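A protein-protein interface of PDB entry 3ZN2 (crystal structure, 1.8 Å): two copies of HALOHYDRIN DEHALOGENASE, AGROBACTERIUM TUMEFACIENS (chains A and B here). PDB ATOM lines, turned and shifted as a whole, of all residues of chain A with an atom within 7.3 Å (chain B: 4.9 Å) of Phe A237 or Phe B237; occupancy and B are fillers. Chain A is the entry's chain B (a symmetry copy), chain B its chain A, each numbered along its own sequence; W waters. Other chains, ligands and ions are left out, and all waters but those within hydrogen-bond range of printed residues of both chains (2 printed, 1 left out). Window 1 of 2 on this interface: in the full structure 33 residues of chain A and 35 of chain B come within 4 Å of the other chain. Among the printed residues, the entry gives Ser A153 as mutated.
Leu A232 touches Leu B220, but with the chains exchanged Leu A220 does not touch Leu B232 (4.2 Å).
Gln A235 touches Val B236, and with the chains exchanged Val A236 touches Gln B235.
Gln A235 touches Phe B237, and with the chains exchanged Phe A237 touches Gln B235.
Phe B237 touches its own counterpart, Phe A237.
Positions printed for both chains: 171, 172, 173, 174, 220, 224, 232, 235, 236, 237, 238 and 239.
Of the 18 pairs that touch across the chains among the printed residues, 14 have their exchanged pair printed and touching as well.
Water W2 bridges O of Trp A238 (2.7 Å) and O of Leu B232 (2.9 Å).
Water W1 lies within hydrogen-bond range of O of Thr A233 (3.3 Å) and O of Trp B238 (3.4 Å).
Among the printed residues, pairs that only touch across the chains: Phe A223 with Leu B220 (3.9 Å), Cys A229 with Leu B220 (3.99 Å), Cys A229 with Leu B239 (3.6 Å), Leu A232 with Leu B220 (3.9 Å), Leu A232 with Phe B237 (3.9 Å), Leu A232 with Trp B238 (3.7 Å), Leu A232 with Leu B239 (3.8 Å), Gln A235 with Phe B237 (3.3 Å), Phe A237 with Leu B232 (3.9 Å), Phe A237 with Gln B235 (3.5 Å), Phe A237 with Phe B237 (3.6 Å), Trp A238 with Leu B232 (3.8 Å) and Leu A239 with Leu B232 (3.8 Å).
Of the 12 printed residues of chain B, 7 touch a printed residue of chain A.
Hydrophobic or aromatic side chains of chain B within 4 Å of the printed part of chain A: Leu B220, Leu B232, Phe B237, Trp B238 and Leu B239.
Along chain B the printed residues that touch a printed residue of chain A span positions 220 to 239.
Of the 25 printed residues of chain A, 8 touch a printed residue of chain B.
Hydrophobic or aromatic side chains of chain A that line the printed part of chain B: Phe A223, Leu A232, Phe A237, Trp A238 and Leu A239.
Among the printed residues, 18 pairs touch across the chains.
Phe A237 touches just these residues of chain B: Leu B232 (3.9 Å), Gln B235 (3.5 Å) and Phe B237 (3.6 Å).
Of chain A, only Leu A232, Gln A235 and Phe A237 come within 4 Å of Phe B237.
Of the printed residues of chain A, Leu B220 touches Phe A223, Cys A229 and Leu A232.
Printed residues of chain B within 4 Å of Val A236: Gln B235 (3.4 Å).
Printed residues of chain B within 4 Å of Leu A232: Leu B220, Phe B237, Trp B238 and Leu B239.
Of the printed residues of chain B, Phe A223 touches Leu B220 (3.9 Å).
The nearest printed residue of chain B that does not touch Phe A237 is Leu B220 (5.9 Å).
The nearest residue of chain A that does not touch Phe B237 is Leu A220 (6.2 Å).
The nearest printed residue of chain A that does not touch Leu B232 is Leu A220 (4.2 Å).
The side-chain amide nitrogen (NE2) of Gln A235 is in hydrogen-bond range of the backbone carbonyl oxygen (O) of Val B236.
NE2 of Gln B235 lies close to NE2 of Gln A235 (3.1 Å).
The backbone NH (N) of Trp B238 lies within hydrogen-bond range of the side-chain amide oxygen (OE1) of Gln A235 (2.7 Å).
N of Trp A238 lies within hydrogen-bond range of OE1 of Gln B235 (2.7 Å).
NE2 of Gln B235 sits at hydrogen-bond distance from O of Val A236, at 3.4 Å.
The backbone NH (N) of Gly B174 is in hydrogen-bond range of the backbone carbonyl oxygen (O) of Phe B237, at 2.6 Å.
The backbone carbonyl oxygen of Gly A174 sits at hydrogen-bond distance from the backbone NH of Leu A239, 3.0 Å away.
N of Leu B239 lies within hydrogen-bond range of O of Gly B174, 3.0 Å away.
N of Ala B172 sits at hydrogen-bond distance from O of Gln B235 (3.1 Å).
The backbone carbonyl oxygen (O) of Ala B172 lies within hydrogen-bond range of the backbone NH (N) of Phe B237 (2.9 Å).
N of Ala A172 sits at hydrogen-bond distance from O of Gln A235, 2.9 Å away.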
ATOM      1  N   ILE A 128      -8.907  -4.793 -18.767  1.00  0.00           N
ATOM      2  CA  ILE A 128      -9.339  -3.647 -17.962  1.00  0.00           C
ATOM      3  C   ILE A 128      -8.191  -2.889 -17.283  1.00  0.00           C
ATOM      4  O   ILE A 128      -7.388  -3.435 -16.483  1.00  0.00           O
ATOM      5  CB  ILE A 128     -10.338  -4.126 -16.955  1.00  0.00           C
ATOM      6  CG1 ILE A 128     -11.465  -4.838 -17.704  1.00  0.00           C
ATOM      7  CG2 ILE A 128     -10.998  -2.933 -16.260  1.00  0.00           C
ATOM      8  CD1 ILE A 128     -12.505  -5.475 -16.822  1.00  0.00           C
ATOM      9  N   PHE A 129      -8.067  -1.622 -17.616  1.00  0.00           N
ATOM     10  CA  PHE A 129      -7.141  -0.710 -16.918  1.00  0.00           C
ATOM     11  C   PHE A 129      -7.914   0.097 -15.901  1.00  0.00           C
ATOM     12  O   PHE A 129      -8.917   0.685 -16.294  1.00  0.00           O
ATOM     13  CB  PHE A 129      -6.502   0.306 -17.818  1.00  0.00           C
ATOM     14  CG  PHE A 129      -5.611  -0.237 -18.862  1.00  0.00           C
ATOM     15  CD1 PHE A 129      -5.242  -1.580 -18.914  1.00  0.00           C
ATOM     16  CD2 PHE A 129      -5.081   0.626 -19.794  1.00  0.00           C
ATOM     17  CE1 PHE A 129      -4.412  -2.054 -19.931  1.00  0.00           C
ATOM     18  CE2 PHE A 129      -4.236   0.169 -20.822  1.00  0.00           C
ATOM     19  CZ  PHE A 129      -3.889  -1.186 -20.873  1.00  0.00           C
ATOM     20  N   THR A 131      -7.707   3.412 -14.351  1.00  0.00           N
ATOM     21  CA  THR A 131      -6.934   4.601 -14.487  1.00  0.00           C
ATOM     22  C   THR A 131      -7.354   5.681 -13.464  1.00  0.00           C
ATOM     23  O   THR A 131      -7.178   5.502 -12.261  1.00  0.00           O
ATOM     24  CB  THR A 131      -6.913   5.096 -15.984  1.00  0.00           C
ATOM     25  OG1 THR A 131      -8.218   5.458 -16.373  1.00  0.00           O
ATOM     26  CG2 THR A 131      -6.388   4.080 -16.939  1.00  0.00           C
ATOM     27  N   SER A 132      -7.788   6.835 -13.943  1.00  0.00           N
ATOM     28  CA  SER A 132      -8.315   7.936 -13.130  1.00  0.00           C
ATOM     29  C   SER A 132      -9.202   8.862 -13.979  1.00  0.00           C
ATOM     30  O   SER A 132      -9.076   8.994 -15.192  1.00  0.00           O
ATOM     31  CB  SER A 132      -7.196   8.780 -12.461  1.00  0.00           C
ATOM     32  OG  SER A 132      -7.754   9.929 -11.776  1.00  0.00           O
ATOM     33  N   ALA A 133     -10.191   9.428 -13.302  1.00  0.00           N
ATOM     34  CA  ALA A 133     -11.038  10.469 -13.863  1.00  0.00           C
ATOM     35  C   ALA A 133     -10.432  11.847 -13.752  1.00  0.00           C
ATOM     36  O   ALA A 133     -11.052  12.843 -14.141  1.00  0.00           O
ATOM     37  CB  ALA A 133     -12.395  10.438 -13.173  1.00  0.00           C
ATOM     38  N   SER A 153      -5.507   5.803 -20.201  1.00  0.00           N
ATOM     39  CA  SER A 153      -6.851   5.696 -20.709  1.00  0.00           C
ATOM     40  C   SER A 153      -6.853   5.678 -22.217  1.00  0.00           C
ATOM     41  O   SER A 153      -7.573   4.889 -22.810  1.00  0.00           O
ATOM     42  CB  SER A 153      -7.795   6.773 -20.106  1.00  0.00           C
ATOM     43  OG  SER A 153      -7.860   6.607 -18.680  1.00  0.00           O
ATOM     44  N   VAL A 170     -11.279  -4.092 -24.646  1.00  0.00           N
ATOM     45  CA  VAL A 170     -10.406  -3.379 -23.858  1.00  0.00           C
ATOM     46  C   VAL A 170     -11.135  -2.119 -23.319  1.00  0.00           C
ATOM     47  O   VAL A 170     -11.724  -1.360 -24.105  1.00  0.00           O
ATOM     48  CB  VAL A 170      -9.239  -2.881 -24.639  1.00  0.00           C
ATOM     49  CG1 VAL A 170      -8.176  -2.370 -23.673  1.00  0.00           C
ATOM     50  CG2 VAL A 170      -8.675  -4.025 -25.518  1.00  0.00           C
ATOM     51  N   PHE A 171     -11.069  -1.983 -22.005  1.00  0.00           N
ATOM     52  CA  PHE A 171     -11.735  -0.943 -21.263  1.00  0.00           C
ATOM     53  C   PHE A 171     -10.805  -0.161 -20.396  1.00  0.00           C
ATOM     54  O   PHE A 171      -9.756  -0.673 -19.853  1.00  0.00           O
ATOM     55  CB  PHE A 171     -12.837  -1.508 -20.390  1.00  0.00           C
ATOM     56  CG  PHE A 171     -13.756  -2.411 -21.090  1.00  0.00           C
ATOM     57  CD1 PHE A 171     -14.826  -1.899 -21.850  1.00  0.00           C
ATOM     58  CD2 PHE A 171     -13.588  -3.789 -20.992  1.00  0.00           C
ATOM     59  CE1 PHE A 171     -15.695  -2.732 -22.523  1.00  0.00           C
ATOM     60  CE2 PHE A 171     -14.461  -4.630 -21.647  1.00  0.00           C
ATOM     61  CZ  PHE A 171     -15.517  -4.114 -22.427  1.00  0.00           C
ATOM     62  N   ALA A 172     -11.125   1.117 -20.191  1.00  0.00           N
ATOM     63  CA  ALA A 172     -10.502   1.789 -19.031  1.00  0.00           C
ATOM     64  C   ALA A 172     -11.605   2.273 -18.051  1.00  0.00           C
ATOM     65  O   ALA A 172     -12.611   2.861 -18.472  1.00  0.00           O
ATOM     66  CB  ALA A 172      -9.595   2.935 -19.416  1.00  0.00           C
ATOM     67  N   ILE A 173     -11.362   2.010 -16.769  1.00  0.00           N
ATOM     68  CA  ILE A 173     -12.126   2.554 -15.708  1.00  0.00           C
ATOM     69  C   ILE A 173     -11.357   3.618 -14.973  1.00  0.00           C
ATOM     70  O   ILE A 173     -10.332   3.363 -14.294  1.00  0.00           O
ATOM     71  CB  ILE A 173     -12.622   1.494 -14.722  1.00  0.00           C
ATOM     72  CG1 ILE A 173     -13.424   0.386 -15.424  1.00  0.00           C
ATOM     73  CG2 ILE A 173     -13.469   2.117 -13.672  1.00  0.00           C
ATOM     74  CD1 ILE A 173     -13.758  -0.845 -14.589  1.00  0.00           C
ATOM     75  N   GLY A 174     -11.873   4.829 -15.091  1.00  0.00           N
ATOM     76  CA  GLY A 174     -11.311   5.999 -14.439  1.00  0.00           C
ATOM     77  C   GLY A 174     -12.045   6.440 -13.170  1.00  0.00           C
ATOM     78  O   GLY A 174     -13.031   7.155 -13.264  1.00  0.00           O
ATOM     79  N   PRO A 175     -11.542   6.057 -11.958  1.00  0.00           N
ATOM     80  CA  PRO A 175     -12.333   6.471 -10.786  1.00  0.00           C
ATOM     81  C   PRO A 175     -11.977   7.824 -10.251  1.00  0.00           C
ATOM     82  O   PRO A 175     -10.889   8.343 -10.558  1.00  0.00           O
ATOM     83  CB  PRO A 175     -11.959   5.405  -9.777  1.00  0.00           C
ATOM     84  CG  PRO A 175     -11.458   4.248 -10.584  1.00  0.00           C
ATOM     85  CD  PRO A 175     -10.630   4.986 -11.586  1.00  0.00           C
ATOM     86  N   LEU A 220     -18.661  -3.459 -11.820  1.00  0.00           N
ATOM     87  CA  LEU A 220     -18.361  -3.057 -13.196  1.00  0.00           C
ATOM     88  C   LEU A 220     -17.327  -3.975 -13.820  1.00  0.00           C
ATOM     89  O   LEU A 220     -17.321  -4.247 -14.976  1.00  0.00           O
ATOM     90  CB  LEU A 220     -17.850  -1.615 -13.172  1.00  0.00           C
ATOM     91  CG  LEU A 220     -17.547  -1.043 -14.575  1.00  0.00           C
ATOM     92  CD1 LEU A 220     -18.725  -1.309 -15.496  1.00  0.00           C
ATOM     93  CD2 LEU A 220     -17.206   0.428 -14.636  1.00  0.00           C
ATOM     94  N   PHE A 223     -18.827  -7.251 -14.626  1.00  0.00           N
ATOM     95  CA  PHE A 223     -19.834  -7.175 -15.690  1.00  0.00           C
ATOM     96  C   PHE A 223     -19.023  -7.087 -16.979  1.00  0.00           C
ATOM     97  O   PHE A 223     -19.309  -7.752 -17.963  1.00  0.00           O
ATOM     98  CB  PHE A 223     -20.716  -5.926 -15.521  1.00  0.00           C
ATOM     99  CG  PHE A 223     -21.585  -5.589 -16.723  1.00  0.00           C
ATOM    100  CD1 PHE A 223     -22.751  -6.281 -16.961  1.00  0.00           C
ATOM    101  CD2 PHE A 223     -21.202  -4.612 -17.627  1.00  0.00           C
ATOM    102  CE1 PHE A 223     -23.505  -6.005 -18.062  1.00  0.00           C
ATOM    103  CE2 PHE A 223     -21.973  -4.320 -18.729  1.00  0.00           C
ATOM    104  CZ  PHE A 223     -23.103  -5.017 -18.922  1.00  0.00           C
ATOM    105  N   LEU A 224     -18.029  -6.231 -16.995  1.00  0.00           N
ATOM    106  CA  LEU A 224     -17.224  -6.143 -18.220  1.00  0.00           C
ATOM    107  C   LEU A 224     -16.423  -7.455 -18.667  1.00  0.00           C
ATOM    108  O   LEU A 224     -16.313  -7.781 -19.882  1.00  0.00           O
ATOM    109  CB  LEU A 224     -16.288  -4.961 -18.156  1.00  0.00           C
ATOM    110  CG  LEU A 224     -16.875  -3.574 -17.958  1.00  0.00           C
ATOM    111  CD1 LEU A 224     -15.777  -2.542 -17.619  1.00  0.00           C
ATOM    112  CD2 LEU A 224     -17.644  -3.163 -19.201  1.00  0.00           C
ATOM    113  N   CYS A 229     -21.227  -7.613 -22.264  1.00  0.00           N
ATOM    114  CA  CYS A 229     -21.341  -6.405 -23.047  1.00  0.00           C
ATOM    115  C   CYS A 229     -20.057  -6.032 -23.700  1.00  0.00           C
ATOM    116  O   CYS A 229     -19.472  -4.957 -23.474  1.00  0.00           O
ATOM    117  CB  CYS A 229     -21.815  -5.272 -22.163  1.00  0.00           C
ATOM    118  SG  CYS A 229     -22.631  -4.000 -23.122  1.00  0.00           S
ATOM    119  N   LEU A 232     -19.159  -2.587 -25.758  1.00  0.00           N
ATOM    120  CA  LEU A 232     -18.709  -1.327 -25.149  1.00  0.00           C
ATOM    121  C   LEU A 232     -17.222  -1.178 -25.309  1.00  0.00           C
ATOM    122  O   LEU A 232     -16.592  -0.217 -24.836  1.00  0.00           O
ATOM    123  CB  LEU A 232     -18.990  -1.276 -23.672  1.00  0.00           C
ATOM    124  CG  LEU A 232     -20.351  -0.959 -23.195  1.00  0.00           C
ATOM    125  CD1 LEU A 232     -20.433  -1.226 -21.659  1.00  0.00           C
ATOM    126  CD2 LEU A 232     -20.676   0.454 -23.556  1.00  0.00           C
ATOM    127  N   THR A 233     -16.604  -2.131 -25.981  1.00  0.00           N
ATOM    128  CA  THR A 233     -15.145  -1.993 -26.161  1.00  0.00           C
ATOM    129  C   THR A 233     -14.638  -0.595 -26.563  1.00  0.00           C
ATOM    130  O   THR A 233     -15.184   0.064 -27.447  1.00  0.00           O
ATOM    131  CB  THR A 233     -14.544  -3.027 -27.179  1.00  0.00           C
ATOM    132  OG1 THR A 233     -13.103  -3.034 -27.028  1.00  0.00           O
ATOM    133  CG2 THR A 233     -14.876  -2.702 -28.566  1.00  0.00           C
ATOM    134  N   GLY A 234     -13.495  -0.267 -25.974  1.00  0.00           N
ATOM    135  CA  GLY A 234     -12.854   1.031 -26.046  1.00  0.00           C
ATOM    136  C   GLY A 234     -13.383   2.075 -25.116  1.00  0.00           C
ATOM    137  O   GLY A 234     -12.901   3.167 -25.149  1.00  0.00           O
ATOM    138  N   GLN A 235     -14.441   1.803 -24.336  1.00  0.00           N
ATOM    139  CA  GLN A 235     -15.022   2.795 -23.396  1.00  0.00           C
ATOM    140  C   GLN A 235     -14.006   3.184 -22.359  1.00  0.00           C
ATOM    141  O   GLN A 235     -13.292   2.275 -21.794  1.00  0.00           O
ATOM    142  CB  GLN A 235     -16.277   2.167 -22.677  1.00  0.00           C
ATOM    143  CG  GLN A 235     -17.090   3.156 -21.853  1.00  0.00           C
ATOM    144  CD  GLN A 235     -17.905   4.147 -22.651  1.00  0.00           C
ATOM    145  OE1 GLN A 235     -18.573   3.835 -23.613  1.00  0.00           O
ATOM    146  NE2 GLN A 235     -17.793   5.395 -22.270  1.00  0.00           N
ATOM    147  N   VAL A 236     -13.922   4.511 -22.083  1.00  0.00           N
ATOM    148  CA  VAL A 236     -13.481   4.976 -20.832  1.00  0.00           C
ATOM    149  C   VAL A 236     -14.687   5.343 -19.912  1.00  0.00           C
ATOM    150  O   VAL A 236     -15.485   6.188 -20.274  1.00  0.00           O
ATOM    151  CB  VAL A 236     -12.545   6.190 -21.018  1.00  0.00           C
ATOM    152  CG1 VAL A 236     -11.884   6.522 -19.684  1.00  0.00           C
ATOM    153  CG2 VAL A 236     -11.502   5.906 -22.124  1.00  0.00           C
ATOM    154  N   PHE A 237     -14.722   4.776 -18.700  1.00  0.00           N
ATOM    155  CA  PHE A 237     -15.788   4.872 -17.761  1.00  0.00           C
ATOM    156  C   PHE A 237     -15.362   5.840 -16.678  1.00  0.00           C
ATOM    157  O   PHE A 237     -14.294   5.706 -16.133  1.00  0.00           O
ATOM    158  CB  PHE A 237     -16.151   3.546 -17.116  1.00  0.00           C
ATOM    159  CG  PHE A 237     -16.592   2.477 -18.032  1.00  0.00           C
ATOM    160  CD1 PHE A 237     -15.678   1.593 -18.602  1.00  0.00           C
ATOM    161  CD2 PHE A 237     -17.963   2.263 -18.287  1.00  0.00           C
ATOM    162  CE1 PHE A 237     -16.088   0.596 -19.414  1.00  0.00           C
ATOM    163  CE2 PHE A 237     -18.373   1.251 -19.074  1.00  0.00           C
ATOM    164  CZ  PHE A 237     -17.425   0.388 -19.659  1.00  0.00           C
ATOM    165  N   TRP A 238     -16.157   6.881 -16.442  1.00  0.00           N
ATOM    166  CA  TRP A 238     -15.876   7.847 -15.445  1.00  0.00           C
ATOM    167  C   TRP A 238     -16.701   7.397 -14.220  1.00  0.00           C
ATOM    168  O   TRP A 238     -17.907   7.631 -14.109  1.00  0.00           O
ATOM    169  CB  TRP A 238     -16.238   9.263 -15.880  1.00  0.00           C
ATOM    170  CG  TRP A 238     -15.540   9.740 -17.151  1.00  0.00           C
ATOM    171  CD1 TRP A 238     -16.159  10.226 -18.296  1.00  0.00           C
ATOM    172  CD2 TRP A 238     -14.123   9.764 -17.419  1.00  0.00           C
ATOM    173  NE1 TRP A 238     -15.199  10.546 -19.245  1.00  0.00           N
ATOM    174  CE2 TRP A 238     -13.952  10.287 -18.733  1.00  0.00           C
ATOM    175  CE3 TRP A 238     -13.002   9.415 -16.685  1.00  0.00           C
ATOM    176  CZ2 TRP A 238     -12.701  10.475 -19.316  1.00  0.00           C
ATOM    177  CZ3 TRP A 238     -11.725   9.561 -17.277  1.00  0.00           C
ATOM    178  CH2 TRP A 238     -11.596  10.127 -18.586  1.00  0.00           C
ATOM    179  N   LEU A 239     -15.973   6.761 -13.318  1.00  0.00           N
ATOM    180  CA  LEU A 239     -16.556   6.131 -12.082  1.00  0.00           C
ATOM    181  C   LEU A 239     -16.316   7.139 -10.925  1.00  0.00           C
ATOM    182  O   LEU A 239     -15.416   6.983 -10.075  1.00  0.00           O
ATOM    183  CB  LEU A 239     -15.917   4.805 -11.796  1.00  0.00           C
ATOM    184  CG  LEU A 239     -16.543   4.021 -10.643  1.00  0.00           C
ATOM    185  CD1 LEU A 239     -17.894   3.508 -11.106  1.00  0.00           C
ATOM    186  CD2 LEU A 239     -15.590   2.901 -10.229  1.00  0.00           C
ATOM    187  N   ALA A 240     -17.070   8.196 -10.988  1.00  0.00           N
ATOM    188  CA  ALA A 240     -16.732   9.422 -10.268  1.00  0.00           C
ATOM    189  C   ALA A 240     -17.939  10.074  -9.602  1.00  0.00           C
ATOM    190  O   ALA A 240     -17.806  11.135  -8.994  1.00  0.00           O
ATOM    191  CB  ALA A 240     -16.049  10.406 -11.182  1.00  0.00           C
ATOM    192  N   PHE B 171     -28.227   8.097 -17.051  1.00  0.00           N
ATOM    193  CA  PHE B 171     -27.222   7.610 -18.024  1.00  0.00           C
ATOM    194  C   PHE B 171     -27.720   7.787 -19.489  1.00  0.00           C
ATOM    195  O   PHE B 171     -28.897   7.775 -19.725  1.00  0.00           O
ATOM    196  CB  PHE B 171     -26.929   6.123 -17.878  1.00  0.00           C
ATOM    197  CG  PHE B 171     -26.629   5.636 -16.459  1.00  0.00           C
ATOM    198  CD1 PHE B 171     -25.353   5.800 -15.895  1.00  0.00           C
ATOM    199  CD2 PHE B 171     -27.615   4.983 -15.739  1.00  0.00           C
ATOM    200  CE1 PHE B 171     -25.101   5.307 -14.632  1.00  0.00           C
ATOM    201  CE2 PHE B 171     -27.360   4.477 -14.456  1.00  0.00           C
ATOM    202  CZ  PHE B 171     -26.084   4.635 -13.924  1.00  0.00           C
ATOM    203  N   ALA B 172     -26.805   7.840 -20.464  1.00  0.00           N
ATOM    204  CA  ALA B 172     -27.149   7.747 -21.860  1.00  0.00           C
ATOM    205  C   ALA B 172     -26.362   6.611 -22.453  1.00  0.00           C
ATOM    206  O   ALA B 172     -25.101   6.542 -22.338  1.00  0.00           O
ATOM    207  CB  ALA B 172     -26.854   9.035 -22.580  1.00  0.00           C
ATOM    208  N   ILE B 173     -27.077   5.732 -23.112  1.00  0.00           N
ATOM    209  CA  ILE B 173     -26.401   4.697 -23.907  1.00  0.00           C
ATOM    210  C   ILE B 173     -26.444   5.055 -25.434  1.00  0.00           C
ATOM    211  O   ILE B 173     -27.527   5.180 -26.011  1.00  0.00           O
ATOM    212  CB  ILE B 173     -27.092   3.375 -23.736  1.00  0.00           C
ATOM    213  CG1 ILE B 173     -27.073   2.931 -22.248  1.00  0.00           C
ATOM    214  CG2 ILE B 173     -26.396   2.277 -24.555  1.00  0.00           C
ATOM    215  CD1 ILE B 173     -27.960   1.691 -22.026  1.00  0.00           C
ATOM    216  N   GLY B 174     -25.309   5.257 -26.063  1.00  0.00           N
ATOM    217  CA  GLY B 174     -25.323   5.715 -27.477  1.00  0.00           C
ATOM    218  C   GLY B 174     -24.877   4.629 -28.446  1.00  0.00           C
ATOM    219  O   GLY B 174     -23.658   4.373 -28.562  1.00  0.00           O
ATOM    220  N   LEU B 220     -26.672  -4.236 -20.485  1.00  0.00           N
ATOM    221  CA  LEU B 220     -26.190  -2.920 -20.010  1.00  0.00           C
ATOM    222  C   LEU B 220     -27.288  -2.149 -19.363  1.00  0.00           C
ATOM    223  O   LEU B 220     -27.122  -1.556 -18.348  1.00  0.00           O
ATOM    224  CB  LEU B 220     -25.581  -2.157 -21.173  1.00  0.00           C
ATOM    225  CG  LEU B 220     -25.029  -0.738 -20.781  1.00  0.00           C
ATOM    226  CD1 LEU B 220     -23.851  -0.745 -19.794  1.00  0.00           C
ATOM    227  CD2 LEU B 220     -24.616  -0.048 -22.028  1.00  0.00           C
ATOM    228  N   LEU B 224     -27.156  -1.236 -15.488  1.00  0.00           N
ATOM    229  CA  LEU B 224     -27.270   0.155 -15.026  1.00  0.00           C
ATOM    230  C   LEU B 224     -28.469   0.439 -14.143  1.00  0.00           C
ATOM    231  O   LEU B 224     -28.328   1.198 -13.235  1.00  0.00           O
ATOM    232  CB  LEU B 224     -27.267   1.144 -16.198  1.00  0.00           C
ATOM    233  CG  LEU B 224     -25.984   1.125 -17.062  1.00  0.00           C
ATOM    234  CD1 LEU B 224     -26.056   2.050 -18.268  1.00  0.00           C
ATOM    235  CD2 LEU B 224     -24.747   1.463 -16.306  1.00  0.00           C
ATOM    236  N   LEU B 232     -21.467   5.512 -11.760  1.00  0.00           N
ATOM    237  CA  LEU B 232     -21.260   5.881 -13.173  1.00  0.00           C
ATOM    238  C   LEU B 232     -22.152   7.031 -13.630  1.00  0.00           C
ATOM    239  O   LEU B 232     -22.100   7.392 -14.791  1.00  0.00           O
ATOM    240  CB  LEU B 232     -21.541   4.661 -14.056  1.00  0.00           C
ATOM    241  CG  LEU B 232     -20.480   3.592 -14.068  1.00  0.00           C
ATOM    242  CD1 LEU B 232     -20.920   2.412 -14.920  1.00  0.00           C
ATOM    243  CD2 LEU B 232     -19.134   4.109 -14.625  1.00  0.00           C
ATOM    244  N   GLN B 235     -22.661   9.226 -17.179  1.00  0.00           N
ATOM    245  CA  GLN B 235     -21.922   8.593 -18.247  1.00  0.00           C
ATOM    246  C   GLN B 235     -22.716   8.474 -19.517  1.00  0.00           C
ATOM    247  O   GLN B 235     -23.809   7.902 -19.577  1.00  0.00           O
ATOM    248  CB  GLN B 235     -21.504   7.160 -17.850  1.00  0.00           C
ATOM    249  CG  GLN B 235     -20.594   6.402 -18.841  1.00  0.00           C
ATOM    250  CD  GLN B 235     -19.195   6.901 -18.757  1.00  0.00           C
ATOM    251  OE1 GLN B 235     -18.580   6.967 -17.713  1.00  0.00           O
ATOM    252  NE2 GLN B 235     -18.660   7.279 -19.904  1.00  0.00           N
ATOM    253  N   VAL B 236     -22.081   8.900 -20.573  1.00  0.00           N
ATOM    254  CA  VAL B 236     -22.490   8.523 -21.932  1.00  0.00           C
ATOM    255  C   VAL B 236     -21.621   7.325 -22.366  1.00  0.00           C
ATOM    256  O   VAL B 236     -20.390   7.401 -22.505  1.00  0.00           O
ATOM    257  CB  VAL B 236     -22.250   9.675 -22.907  1.00  0.00           C
ATOM    258  CG1 VAL B 236     -22.760   9.282 -24.299  1.00  0.00           C
ATOM    259  CG2 VAL B 236     -22.896  10.957 -22.422  1.00  0.00           C
ATOM    260  N   PHE B 237     -22.277   6.242 -22.628  1.00  0.00           N
ATOM    261  CA  PHE B 237     -21.677   4.953 -23.056  1.00  0.00           C
ATOM    262  C   PHE B 237     -21.747   4.810 -24.559  1.00  0.00           C
ATOM    263  O   PHE B 237     -22.853   4.891 -25.164  1.00  0.00           O
ATOM    264  CB  PHE B 237     -22.501   3.805 -22.543  1.00  0.00           C
ATOM    265  CG  PHE B 237     -22.570   3.718 -21.067  1.00  0.00           C
ATOM    266  CD1 PHE B 237     -21.581   3.026 -20.334  1.00  0.00           C
ATOM    267  CD2 PHE B 237     -23.572   4.357 -20.400  1.00  0.00           C
ATOM    268  CE1 PHE B 237     -21.622   2.902 -18.963  1.00  0.00           C
ATOM    269  CE2 PHE B 237     -23.629   4.231 -19.000  1.00  0.00           C
ATOM    270  CZ  PHE B 237     -22.645   3.553 -18.288  1.00  0.00           C
ATOM    271  N   TRP B 238     -20.626   4.553 -25.186  1.00  0.00           N
ATOM    272  CA  TRP B 238     -20.591   4.340 -26.636  1.00  0.00           C
ATOM    273  C   TRP B 238     -20.712   2.827 -26.911  1.00  0.00           C
ATOM    274  O   TRP B 238     -19.743   2.043 -26.800  1.00  0.00           O
ATOM    275  CB  TRP B 238     -19.271   4.912 -27.194  1.00  0.00           C
ATOM    276  CG  TRP B 238     -19.061   6.312 -26.877  1.00  0.00           C
ATOM    277  CD1 TRP B 238     -17.925   6.866 -26.320  1.00  0.00           C
ATOM    278  CD2 TRP B 238     -19.939   7.417 -27.161  1.00  0.00           C
ATOM    279  NE1 TRP B 238     -18.069   8.235 -26.223  1.00  0.00           N
ATOM    280  CE2 TRP B 238     -19.288   8.596 -26.722  1.00  0.00           C
ATOM    281  CE3 TRP B 238     -21.226   7.533 -27.713  1.00  0.00           C
ATOM    282  CZ2 TRP B 238     -19.875   9.833 -26.816  1.00  0.00           C
ATOM    283  CZ3 TRP B 238     -21.779   8.761 -27.834  1.00  0.00           C
ATOM    284  CH2 TRP B 238     -21.106   9.906 -27.385  1.00  0.00           C
ATOM    285  N   LEU B 239     -21.908   2.387 -27.217  1.00  0.00           N
ATOM    286  CA  LEU B 239     -22.114   0.986 -27.472  1.00  0.00           C
ATOM    287  C   LEU B 239     -22.035   0.712 -28.999  1.00  0.00           C
ATOM    288  O   LEU B 239     -23.051   0.556 -29.679  1.00  0.00           O
ATOM    289  CB  LEU B 239     -23.433   0.605 -26.867  1.00  0.00           C
ATOM    290  CG  LEU B 239     -23.716  -0.921 -26.911  1.00  0.00           C
ATOM    291  CD1 LEU B 239     -22.917  -1.716 -25.908  1.00  0.00           C
ATOM    292  CD2 LEU B 239     -25.198  -1.155 -26.540  1.00  0.00           C
HETATM  293  O   HOH W   1     -17.543   1.412 -29.262  1.00  0.00           O
HETATM  294  O   HOH W   2     -19.829   9.190 -15.069  1.00  0.00           O
